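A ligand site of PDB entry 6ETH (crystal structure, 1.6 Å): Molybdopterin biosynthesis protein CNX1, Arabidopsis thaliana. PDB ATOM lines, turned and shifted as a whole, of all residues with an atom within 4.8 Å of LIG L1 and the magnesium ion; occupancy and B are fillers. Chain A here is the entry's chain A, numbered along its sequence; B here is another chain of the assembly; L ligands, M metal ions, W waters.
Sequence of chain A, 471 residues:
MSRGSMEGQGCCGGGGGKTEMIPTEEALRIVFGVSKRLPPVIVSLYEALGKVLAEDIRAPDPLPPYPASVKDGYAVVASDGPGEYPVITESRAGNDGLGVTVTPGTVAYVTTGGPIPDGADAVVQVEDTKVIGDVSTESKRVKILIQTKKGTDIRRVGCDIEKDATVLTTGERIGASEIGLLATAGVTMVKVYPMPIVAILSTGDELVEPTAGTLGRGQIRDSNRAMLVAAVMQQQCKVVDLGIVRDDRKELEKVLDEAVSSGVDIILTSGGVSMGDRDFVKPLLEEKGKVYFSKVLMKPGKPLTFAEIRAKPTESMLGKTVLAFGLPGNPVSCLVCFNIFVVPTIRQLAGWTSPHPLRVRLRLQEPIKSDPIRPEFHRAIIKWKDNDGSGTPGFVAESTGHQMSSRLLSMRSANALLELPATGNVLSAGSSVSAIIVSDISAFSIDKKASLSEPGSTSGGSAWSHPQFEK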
ATOM      1  N   SER A 202     -33.151  -5.232   7.374  1.00  0.00           N
ATOM      2  CA  SER A 202     -31.746  -5.538   7.111  1.00  0.00           C
ATOM      3  C   SER A 202     -31.116  -5.967   8.411  1.00  0.00           C
ATOM      4  O   SER A 202     -31.567  -5.571   9.490  1.00  0.00           O
ATOM      5  CB  SER A 202     -31.000  -4.314   6.589  1.00  0.00           C
ATOM      6  OG  SER A 202     -31.248  -4.128   5.206  1.00  0.00           O
ATOM      7  N   THR A 203     -30.048  -6.762   8.314  1.00  0.00           N
ATOM      8  CA  THR A 203     -29.341  -7.162   9.533  1.00  0.00           C
ATOM      9  C   THR A 203     -27.854  -6.813   9.446  1.00  0.00           C
ATOM     10  O   THR A 203     -27.253  -6.940   8.378  1.00  0.00           O
ATOM     11  CB  THR A 203     -29.517  -8.662   9.832  1.00  0.00           C
ATOM     12  OG1 THR A 203     -28.780  -9.441   8.871  1.00  0.00           O
ATOM     13  CG2 THR A 203     -31.006  -9.091   9.885  1.00  0.00           C
ATOM     14  N   GLY A 204     -27.284  -6.412  10.577  1.00  0.00           N
ATOM     15  CA  GLY A 204     -25.833  -6.234  10.623  1.00  0.00           C
ATOM     16  C   GLY A 204     -25.310  -5.151  11.530  1.00  0.00           C
ATOM     17  O   GLY A 204     -25.710  -3.991  11.435  1.00  0.00           O
ATOM     18  N   GLU A 206     -22.437  -3.924  11.104  1.00  0.00           N
ATOM     19  CA  GLU A 206     -21.637  -3.066  10.215  1.00  0.00           C
ATOM     20  C   GLU A 206     -22.490  -2.054   9.436  1.00  0.00           C
ATOM     21  O   GLU A 206     -21.926  -1.178   8.800  1.00  0.00           O
ATOM     22  CB  GLU A 206     -20.766  -3.899   9.254  1.00  0.00           C
ATOM     23  CG  GLU A 206     -21.461  -4.519   8.043  1.00  0.00           C
ATOM     24  CD  GLU A 206     -22.335  -5.742   8.254  1.00  0.00           C
ATOM     25  OE1 GLU A 206     -22.648  -6.074   9.419  1.00  0.00           O
ATOM     26  OE2 GLU A 206     -22.704  -6.374   7.242  1.00  0.00           O
ATOM     27  N   LEU A 207     -23.818  -2.158   9.476  1.00  0.00           N
ATOM     28  CA  LEU A 207     -24.658  -1.269   8.665  1.00  0.00           C
ATOM     29  C   LEU A 207     -24.909   0.073   9.295  1.00  0.00           C
ATOM     30  O   LEU A 207     -25.044   0.159  10.518  1.00  0.00           O
ATOM     31  CB  LEU A 207     -26.034  -1.945   8.436  1.00  0.00           C
ATOM     32  CG  LEU A 207     -26.018  -3.327   7.775  1.00  0.00           C
ATOM     33  CD1 LEU A 207     -27.447  -3.825   7.598  1.00  0.00           C
ATOM     34  CD2 LEU A 207     -25.284  -3.299   6.431  1.00  0.00           C
ATOM     35  N   ILE A 220     -20.677   0.229   6.517  1.00  0.00           N
ATOM     36  CA  ILE A 220     -21.145   0.371   5.155  1.00  0.00           C
ATOM     37  C   ILE A 220     -22.585   0.879   5.214  1.00  0.00           C
ATOM     38  O   ILE A 220     -23.273   0.572   6.186  1.00  0.00           O
ATOM     39  CB  ILE A 220     -21.076  -0.928   4.331  1.00  0.00           C
ATOM     40  CG1 ILE A 220     -21.938  -2.068   4.947  1.00  0.00           C
ATOM     41  CG2 ILE A 220     -19.651  -1.351   4.143  1.00  0.00           C
ATOM     42  CD1 ILE A 220     -22.188  -3.254   3.957  1.00  0.00           C
ATOM     43  N   ARG A 221     -23.064   1.549   4.167  1.00  0.00           N
ATOM     44  CA  ARG A 221     -24.473   1.966   4.135  1.00  0.00           C
ATOM     45  C   ARG A 221     -25.346   0.751   3.845  1.00  0.00           C
ATOM     46  O   ARG A 221     -24.991  -0.097   3.009  1.00  0.00           O
ATOM     47  CB  ARG A 221     -24.731   3.019   3.031  1.00  0.00           C
ATOM     48  CG  ARG A 221     -23.926   4.316   3.317  1.00  0.00           C
ATOM     49  CD  ARG A 221     -24.248   5.520   2.430  1.00  0.00           C
ATOM     50  NE  ARG A 221     -23.289   6.593   2.739  1.00  0.00           N
ATOM     51  CZ  ARG A 221     -22.048   6.680   2.258  1.00  0.00           C
ATOM     52  NH1 ARG A 221     -21.621   5.827   1.340  1.00  0.00           N
ATOM     53  NH2 ARG A 221     -21.234   7.636   2.698  1.00  0.00           N
ATOM     54  N   ASP A 222     -26.507   0.675   4.507  1.00  0.00           N
ATOM     55  CA  ASP A 222     -27.500  -0.370   4.242  1.00  0.00           C
ATOM     56  C   ASP A 222     -28.052  -0.084   2.820  1.00  0.00           C
ATOM     57  O   ASP A 222     -28.778   0.899   2.635  1.00  0.00           O
ATOM     58  CB  ASP A 222     -28.635  -0.240   5.275  1.00  0.00           C
ATOM     59  CG  ASP A 222     -29.830  -1.147   5.101  1.00  0.00           C
ATOM     60  OD1 ASP A 222     -29.789  -2.038   4.226  1.00  0.00           O
ATOM     61  OD2 ASP A 222     -30.793  -0.976   5.844  1.00  0.00           O
ATOM     62  N   SER A 223     -27.687  -0.918   1.814  1.00  0.00           N
ATOM     63  CA  SER A 223     -28.216  -0.755   0.460  1.00  0.00           C
ATOM     64  C   SER A 223     -29.338  -1.796   0.155  1.00  0.00           C
ATOM     65  O   SER A 223     -30.232  -1.513  -0.653  1.00  0.00           O
ATOM     66  CB  SER A 223     -27.098  -0.897  -0.586  1.00  0.00           C
ATOM     67  OG  SER A 223     -26.501  -2.175  -0.532  1.00  0.00           O
ATOM     68  N   ASN A 224     -29.297  -3.004   0.768  1.00  0.00           N
ATOM     69  CA  ASN A 224     -30.308  -4.043   0.475  1.00  0.00           C
ATOM     70  C   ASN A 224     -31.725  -3.620   0.804  1.00  0.00           C
ATOM     71  O   ASN A 224     -32.649  -3.965   0.070  1.00  0.00           O
ATOM     72  CB  ASN A 224     -30.019  -5.352   1.236  1.00  0.00           C
ATOM     73  CG  ASN A 224     -28.805  -6.122   0.752  1.00  0.00           C
ATOM     74  OD1 ASN A 224     -28.240  -5.820  -0.291  1.00  0.00           O
ATOM     75  ND2 ASN A 224     -28.378  -7.109   1.518  1.00  0.00           N
ATOM     76  N   ARG A 225     -31.918  -2.906   1.923  1.00  0.00           N
ATOM     77  CA  ARG A 225     -33.269  -2.566   2.337  1.00  0.00           C
ATOM     78  C   ARG A 225     -33.953  -1.659   1.315  1.00  0.00           C
ATOM     79  O   ARG A 225     -35.039  -2.013   0.824  1.00  0.00           O
ATOM     80  CB  ARG A 225     -33.267  -1.927   3.737  1.00  0.00           C
ATOM     81  CG  ARG A 225     -34.679  -1.641   4.315  1.00  0.00           C
ATOM     82  CD  ARG A 225     -34.593  -1.562   5.832  1.00  0.00           C
ATOM     83  NE  ARG A 225     -33.484  -0.698   6.231  1.00  0.00           N
ATOM     84  CZ  ARG A 225     -33.540   0.610   6.478  1.00  0.00           C
ATOM     85  NH1 ARG A 225     -34.721   1.233   6.546  1.00  0.00           N
ATOM     86  NH2 ARG A 225     -32.440   1.283   6.750  1.00  0.00           N
ATOM     87  N   ASP A 247     -26.889  -7.618  15.083  1.00  0.00           N
ATOM     88  CA  ASP A 247     -26.604  -9.056  15.204  1.00  0.00           C
ATOM     89  C   ASP A 247     -26.708  -9.477  16.682  1.00  0.00           C
ATOM     90  O   ASP A 247     -25.721  -9.781  17.333  1.00  0.00           O
ATOM     91  CB  ASP A 247     -25.209  -9.367  14.610  1.00  0.00           C
ATOM     92  CG  ASP A 247     -25.110  -8.995  13.128  1.00  0.00           C
ATOM     93  OD1 ASP A 247     -26.071  -9.284  12.372  1.00  0.00           O
ATOM     94  OD2 ASP A 247     -24.100  -8.396  12.741  1.00  0.00           O
ATOM     95  N   SER A 270     -32.431  -9.710   5.085  1.00  0.00           N
ATOM     96  CA  SER A 270     -31.222  -9.972   4.304  1.00  0.00           C
ATOM     97  C   SER A 270     -30.075 -10.030   5.292  1.00  0.00           C
ATOM     98  O   SER A 270     -30.168  -9.478   6.384  1.00  0.00           O
ATOM     99  CB  SER A 270     -30.995  -8.945   3.174  1.00  0.00           C
ATOM    100  OG  SER A 270     -30.494  -7.685   3.599  1.00  0.00           O
ATOM    101  N   GLY A 271     -29.069 -10.808   4.972  1.00  0.00           N
ATOM    102  CA  GLY A 271     -27.921 -10.988   5.852  1.00  0.00           C
ATOM    103  C   GLY A 271     -28.211 -11.918   7.011  1.00  0.00           C
ATOM    104  O   GLY A 271     -29.324 -12.421   7.146  1.00  0.00           O
ATOM    105  N   GLY A 272     -27.201 -12.167   7.849  1.00  0.00           N
ATOM    106  CA  GLY A 272     -27.366 -13.004   9.038  1.00  0.00           C
ATOM    107  C   GLY A 272     -27.643 -14.469   8.778  1.00  0.00           C
ATOM    108  O   GLY A 272     -28.175 -15.150   9.659  1.00  0.00           O
ATOM    109  N   VAL A 273     -27.340 -14.961   7.551  1.00  0.00           N
ATOM    110  CA  VAL A 273     -27.564 -16.339   7.110  1.00  0.00           C
ATOM    111  C   VAL A 273     -26.246 -16.981   6.659  1.00  0.00           C
ATOM    112  O   VAL A 273     -26.306 -18.003   5.975  1.00  0.00           O
ATOM    113  CB  VAL A 273     -28.666 -16.454   6.008  1.00  0.00           C
ATOM    114  CG1 VAL A 273     -30.050 -16.160   6.580  1.00  0.00           C
ATOM    115  CG2 VAL A 273     -28.370 -15.560   4.811  1.00  0.00           C
ATOM    116  N   SER A 274     -25.064 -16.422   7.021  1.00  0.00           N
ATOM    117  CA  SER A 274     -23.776 -17.032   6.667  1.00  0.00           C
ATOM    118  C   SER A 274     -23.352 -17.995   7.810  1.00  0.00           C
ATOM    119  O   SER A 274     -24.216 -18.512   8.518  1.00  0.00           O
ATOM    120  CB  SER A 274     -22.726 -15.970   6.343  1.00  0.00           C
ATOM    121  OG  SER A 274     -23.164 -15.150   5.265  1.00  0.00           O
ATOM    122  N   ASP A 279     -24.899 -14.945  13.405  1.00  0.00           N
ATOM    123  CA  ASP A 279     -25.867 -15.068  12.293  1.00  0.00           C
ATOM    124  C   ASP A 279     -27.051 -15.839  12.867  1.00  0.00           C
ATOM    125  O   ASP A 279     -26.958 -17.054  13.045  1.00  0.00           O
ATOM    126  CB  ASP A 279     -25.236 -15.852  11.119  1.00  0.00           C
ATOM    127  CG  ASP A 279     -24.299 -14.999  10.274  1.00  0.00           C
ATOM    128  OD1 ASP A 279     -24.382 -13.775  10.370  1.00  0.00           O
ATOM    129  OD2 ASP A 279     -23.482 -15.569   9.558  1.00  0.00           O
ATOM    130  N   PRO A 328     -29.803 -13.814   1.198  1.00  0.00           N
ATOM    131  CA  PRO A 328     -28.366 -13.606   1.487  1.00  0.00           C
ATOM    132  C   PRO A 328     -28.043 -12.110   1.622  1.00  0.00           C
ATOM    133  O   PRO A 328     -28.673 -11.266   0.979  1.00  0.00           O
ATOM    134  CB  PRO A 328     -27.650 -14.203   0.275  1.00  0.00           C
ATOM    135  CG  PRO A 328     -28.688 -14.984  -0.471  1.00  0.00           C
ATOM    136  CD  PRO A 328     -30.009 -14.413  -0.129  1.00  0.00           C
ATOM    137  N   GLY A 329     -27.045 -11.777   2.444  1.00  0.00           N
ATOM    138  CA  GLY A 329     -26.651 -10.369   2.616  1.00  0.00           C
ATOM    139  C   GLY A 329     -25.941  -9.770   1.407  1.00  0.00           C
ATOM    140  O   GLY A 329     -26.013  -8.562   1.192  1.00  0.00           O
ATOM    141  N   ASN A 330     -25.160 -10.578   0.656  1.00  0.00           N
ATOM    142  CA  ASN A 330     -24.440 -10.017  -0.502  1.00  0.00           C
ATOM    143  C   ASN A 330     -25.421  -9.355  -1.463  1.00  0.00           C
ATOM    144  O   ASN A 330     -26.385 -10.013  -1.858  1.00  0.00           O
ATOM    145  CB  ASN A 330     -23.598 -11.086  -1.221  1.00  0.00           C
ATOM    146  CG  ASN A 330     -22.238 -11.274  -0.573  1.00  0.00           C
ATOM    147  OD1 ASN A 330     -21.431 -10.343  -0.473  1.00  0.00           O
ATOM    148  ND2 ASN A 330     -21.954 -12.459  -0.063  1.00  0.00           N
ATOM    149  N   PRO A 331     -25.254  -8.052  -1.814  1.00  0.00           N
ATOM    150  CA  PRO A 331     -26.283  -7.347  -2.628  1.00  0.00           C
ATOM    151  C   PRO A 331     -26.757  -8.054  -3.892  1.00  0.00           C
ATOM    152  O   PRO A 331     -27.930  -8.070  -4.162  1.00  0.00           O
ATOM    153  CB  PRO A 331     -25.592  -6.029  -2.963  1.00  0.00           C
ATOM    154  CG  PRO A 331     -24.820  -5.727  -1.722  1.00  0.00           C
ATOM    155  CD  PRO A 331     -24.233  -7.079  -1.340  1.00  0.00           C
ATOM    156  N   THR B 112     -18.155 -12.715   7.809  1.00  0.00           N
ATOM    157  CA  THR B 112     -18.303 -12.130   6.473  1.00  0.00           C
ATOM    158  C   THR B 112     -18.593 -10.649   6.603  1.00  0.00           C
ATOM    159  O   THR B 112     -19.398 -10.260   7.429  1.00  0.00           O
ATOM    160  CB  THR B 112     -19.402 -12.866   5.663  1.00  0.00           C
ATOM    161  OG1 THR B 112     -19.124 -14.271   5.726  1.00  0.00           O
ATOM    162  CG2 THR B 112     -19.442 -12.451   4.227  1.00  0.00           C
ATOM    163  N   GLY B 113     -17.876  -9.819   5.860  1.00  0.00           N
ATOM    164  CA  GLY B 113     -17.993  -8.370   5.951  1.00  0.00           C
ATOM    165  C   GLY B 113     -17.216  -7.747   7.104  1.00  0.00           C
ATOM    166  O   GLY B 113     -17.206  -6.533   7.239  1.00  0.00           O
ATOM    167  N   ARG B 155     -11.860  -8.830   0.369  1.00  0.00           N
ATOM    168  CA  ARG B 155     -12.305  -7.820  -0.574  1.00  0.00           C
ATOM    169  C   ARG B 155     -11.470  -6.599  -0.240  1.00  0.00           C
ATOM    170  O   ARG B 155     -11.717  -5.984   0.808  1.00  0.00           O
ATOM    171  CB  ARG B 155     -13.800  -7.492  -0.373  1.00  0.00           C
ATOM    172  CG  ARG B 155     -14.705  -8.543  -0.975  1.00  0.00           C
ATOM    173  CD  ARG B 155     -16.116  -8.481  -0.395  1.00  0.00           C
ATOM    174  NE  ARG B 155     -16.724  -7.183  -0.716  1.00  0.00           N
ATOM    175  CZ  ARG B 155     -17.414  -6.417   0.128  1.00  0.00           C
ATOM    176  NH1 ARG B 155     -17.654  -6.803   1.372  1.00  0.00           N
ATOM    177  NH2 ARG B 155     -17.889  -5.248  -0.286  1.00  0.00           N
HETATM  178  P1  LIG L   1     -24.124 -11.684   5.992  1.00  0.00           P
HETATM  179  O1  LIG L   1     -22.890 -12.401   6.450  1.00  0.00           O
HETATM  180  O2  LIG L   1     -24.774 -10.891   7.122  1.00  0.00           O
HETATM  181  O3  LIG L   1     -25.038 -12.505   5.148  1.00  0.00           O
HETATM  182  O4  LIG L   1     -23.592 -10.644   4.906  1.00  0.00           O
HETATM  183  C1  LIG L   1     -22.919 -11.050   3.712  1.00  0.00           C
HETATM  184  C2  LIG L   1     -22.253  -9.832   3.087  1.00  0.00           C
HETATM  185  O5  LIG L   1     -23.288  -8.905   2.643  1.00  0.00           O
HETATM  186  C3  LIG L   1     -21.330  -9.024   4.028  1.00  0.00           C
HETATM  187  O6  LIG L   1     -20.219  -8.525   3.279  1.00  0.00           O
HETATM  188  C4  LIG L   1     -22.222  -7.896   4.497  1.00  0.00           C
HETATM  189  O7  LIG L   1     -21.524  -6.731   4.945  1.00  0.00           O
HETATM  190  C5  LIG L   1     -23.103  -7.651   3.273  1.00  0.00           C
HETATM  191  N1  LIG L   1     -24.424  -7.117   3.685  1.00  0.00           N
HETATM  192  C6  LIG L   1     -25.290  -7.637   4.588  1.00  0.00           C
HETATM  193  N2  LIG L   1     -26.403  -6.874   4.675  1.00  0.00           N
HETATM  194  C7  LIG L   1     -26.250  -5.845   3.820  1.00  0.00           C
HETATM  195  C8  LIG L   1     -27.029  -4.642   3.448  1.00  0.00           C
HETATM  196  N3  LIG L   1     -28.228  -4.418   3.990  1.00  0.00           N
HETATM  197  N4  LIG L   1     -26.528  -3.823   2.496  1.00  0.00           N
HETATM  198  C9  LIG L   1     -25.337  -4.045   1.908  1.00  0.00           C
HETATM  199  N5  LIG L   1     -24.560  -5.119   2.218  1.00  0.00           N
HETATM  200  C10 LIG L   1     -24.952  -6.015   3.148  1.00  0.00           C
HETATM  201  C1  LG2 L   2     -20.795 -10.173  10.191  1.00  0.00           C
HETATM  202  O1  LG2 L   2     -20.988 -11.073   9.386  1.00  0.00           O
HETATM  203  C2  LG2 L   2     -20.194  -8.825   9.855  1.00  0.00           C
HETATM  204 MG    MG M   1     -24.203  -9.735   8.584  1.00  0.00          MG
HETATM  205  O   HOH W   1     -22.336  -4.282   0.545  1.00  0.00           O
HETATM  206  O   HOH W   2     -25.447 -14.272   3.375  1.00  0.00           O
HETATM  207  O   HOH W   3     -17.851  -9.604   2.421  1.00  0.00           O
HETATM  208  O   HOH W   4     -20.738  -7.958   0.578  1.00  0.00           O
HETATM  209  O   HOH W   5     -29.008  -6.800   5.664  1.00  0.00           O
HETATM  210  O   HOH W   6     -19.043  -5.532   3.880  1.00  0.00           O
HETATM  211  O   HOH W   7     -24.790  -7.960   7.687  1.00  0.00           O
HETATM  212  O   HOH W   8     -26.033  -9.849   9.575  1.00  0.00           O
HETATM  213  O   HOH W   9     -23.369  -8.631  10.068  1.00  0.00           O
HETATM  214  O   HOH W  10     -23.583 -11.465   9.613  1.00  0.00           O
HETATM  215  O   HOH W  11     -22.340  -9.449   7.638  1.00  0.00           O
HETATM  216  O   HOH W  12     -21.383 -13.844   9.242  1.00  0.00           O
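An oxygen (O7) of LIG L1 sits at hydrogen-bond distance from the side-chain carboxylate (OE2) of Glu 206 (2.6 Å). The backbone NH of Gly 272 lies within hydrogen-bond range of an oxygen (O3) of LIG L1 (3.5 Å). A nitrogen (N3) of LIG L1 is in hydrogen-bond range of the side-chain carboxylate of Asp 222 (2.9 Å). OG of Ser 274 is in hydrogen-bond range of O1 of LIG L1. N of Gly 329 sits at hydrogen-bond distance from O3 of LIG L1, 3.4 Å away. N4 of LIG L1 sits at hydrogen-bond distance from N of Ser 223, at 3.2 Å. A nitrogen (N4) of LIG L1 lies close to the side-chain hydroxyl (OG) of Ser 223. The backbone NH of Asn 330 is in hydrogen-bond range of an oxygen (O5) of LIG L1 (3.2 Å). N3 of LIG L1 is in hydrogen-bond range of OG of Ser 202, at 3.3 Å. A nitrogen (N4) of LIG L1 lies within hydrogen-bond range of the backbone NH (N) of Asn 224, 3.4 Å away. O of Thr 112 of chain B lies close to O1 of LG2 L2 (2.6 Å).
The backbone carbonyl oxygen (O) of Glu 206 lies within hydrogen-bond range of the backbone NH (N) of Ile 220, 3.0 Å away. The side-chain hydroxyl of Thr 203 sits at hydrogen-bond distance from the backbone NH of Gly 272 (3.3 Å). OD1 of Asp 222 sits at hydrogen-bond distance from OG of Ser 202 (2.7 Å). The side-chain carboxylate (OD2) of Asp 222 is in salt-bridge range of the guanidinium group (NE) of Arg 225, at 2.7 Å. The side-chain carboxylate of Asp 279 lies close to the backbone NH of Ser 274 (3.1 Å). The backbone carbonyl oxygen of Gly 329 is in hydrogen-bond range of the side-chain amide nitrogen of Asn 224 (2.8 Å). OG1 of Thr 203 lies close to O of Gly 271 (3.5 Å). The side-chain hydroxyl of Thr 203 lies within hydrogen-bond range of the backbone carbonyl oxygen of Ser 270.
Thr 203 touches LIG L1. Leu 207 touches LIG L1. Ile 220 touches LIG L1. Ser 270 touches LIG L1 (OG to N3, 3.995 Å). Gly 271 touches LIG L1 (CA to O3, 3.3 Å). Pro 331 touches LIG L1 (CG to N5, 3.995 Å). CB of Thr 112 of chain B touches O1 of LIG L1, at 3.6 Å. Gly 113 of chain B touches LIG L1. Arg 155 of chain B touches LIG L1 (NH1 to O6, 3.6 Å). Of the 25 residues printed, 18 come within 4 Å of LIG L1.
OE2 of Glu 206 touches the magnesium ion, 3.9 Å away. Gly 272 touches the magnesium ion. Of the 25 residues printed, 2 come within 4 Å of the magnesium ion.
The magnesium ion is bound by O2 of LIG L1 (1.9 Å), water W9 (2.0 Å), water W7 (2.1 Å), water W8 (2.1 Å), water W10 (2.1 Å) and water W11 (2.1 Å).
Water W8 lies within hydrogen-bond range of OD1 of Asp 247 (2.9 Å), OG1 of Thr 203 (2.9 Å) and N of Gly 272 (3.1 Å). Water W10 lies within hydrogen-bond range of the side-chain carboxylate (OD1) of Asp 279 (2.6 Å), an oxygen (O1) of LG2 L2 (2.6 Å) and an oxygen (O1) of LIG L1 (3.4 Å). Water W2 lies within hydrogen-bond range of O3 of LIG L1 (2.5 Å), OG of Ser 274 (3.1 Å) and N of Gly 329 (3.1 Å). Water W3 lies within hydrogen-bond range of O6 of LIG L1 (2.7 Å), NH1 of Arg 155 of chain B (3.0 Å) and N of Gly 113 of chain B (3.4 Å). Water W4 lies within hydrogen-bond range of OD1 of Asn 330 (2.7 Å), O6 of LIG L1 (2.8 Å) and NH1 of Arg 155 of chain B (3.4 Å). Water W12 lies within hydrogen-bond range of the side-chain carboxylate of Asp 279 (2.7 Å), an oxygen (O1) of LG2 L2 (2.8 Å) and an oxygen (O1) of LIG L1 (3.5 Å).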
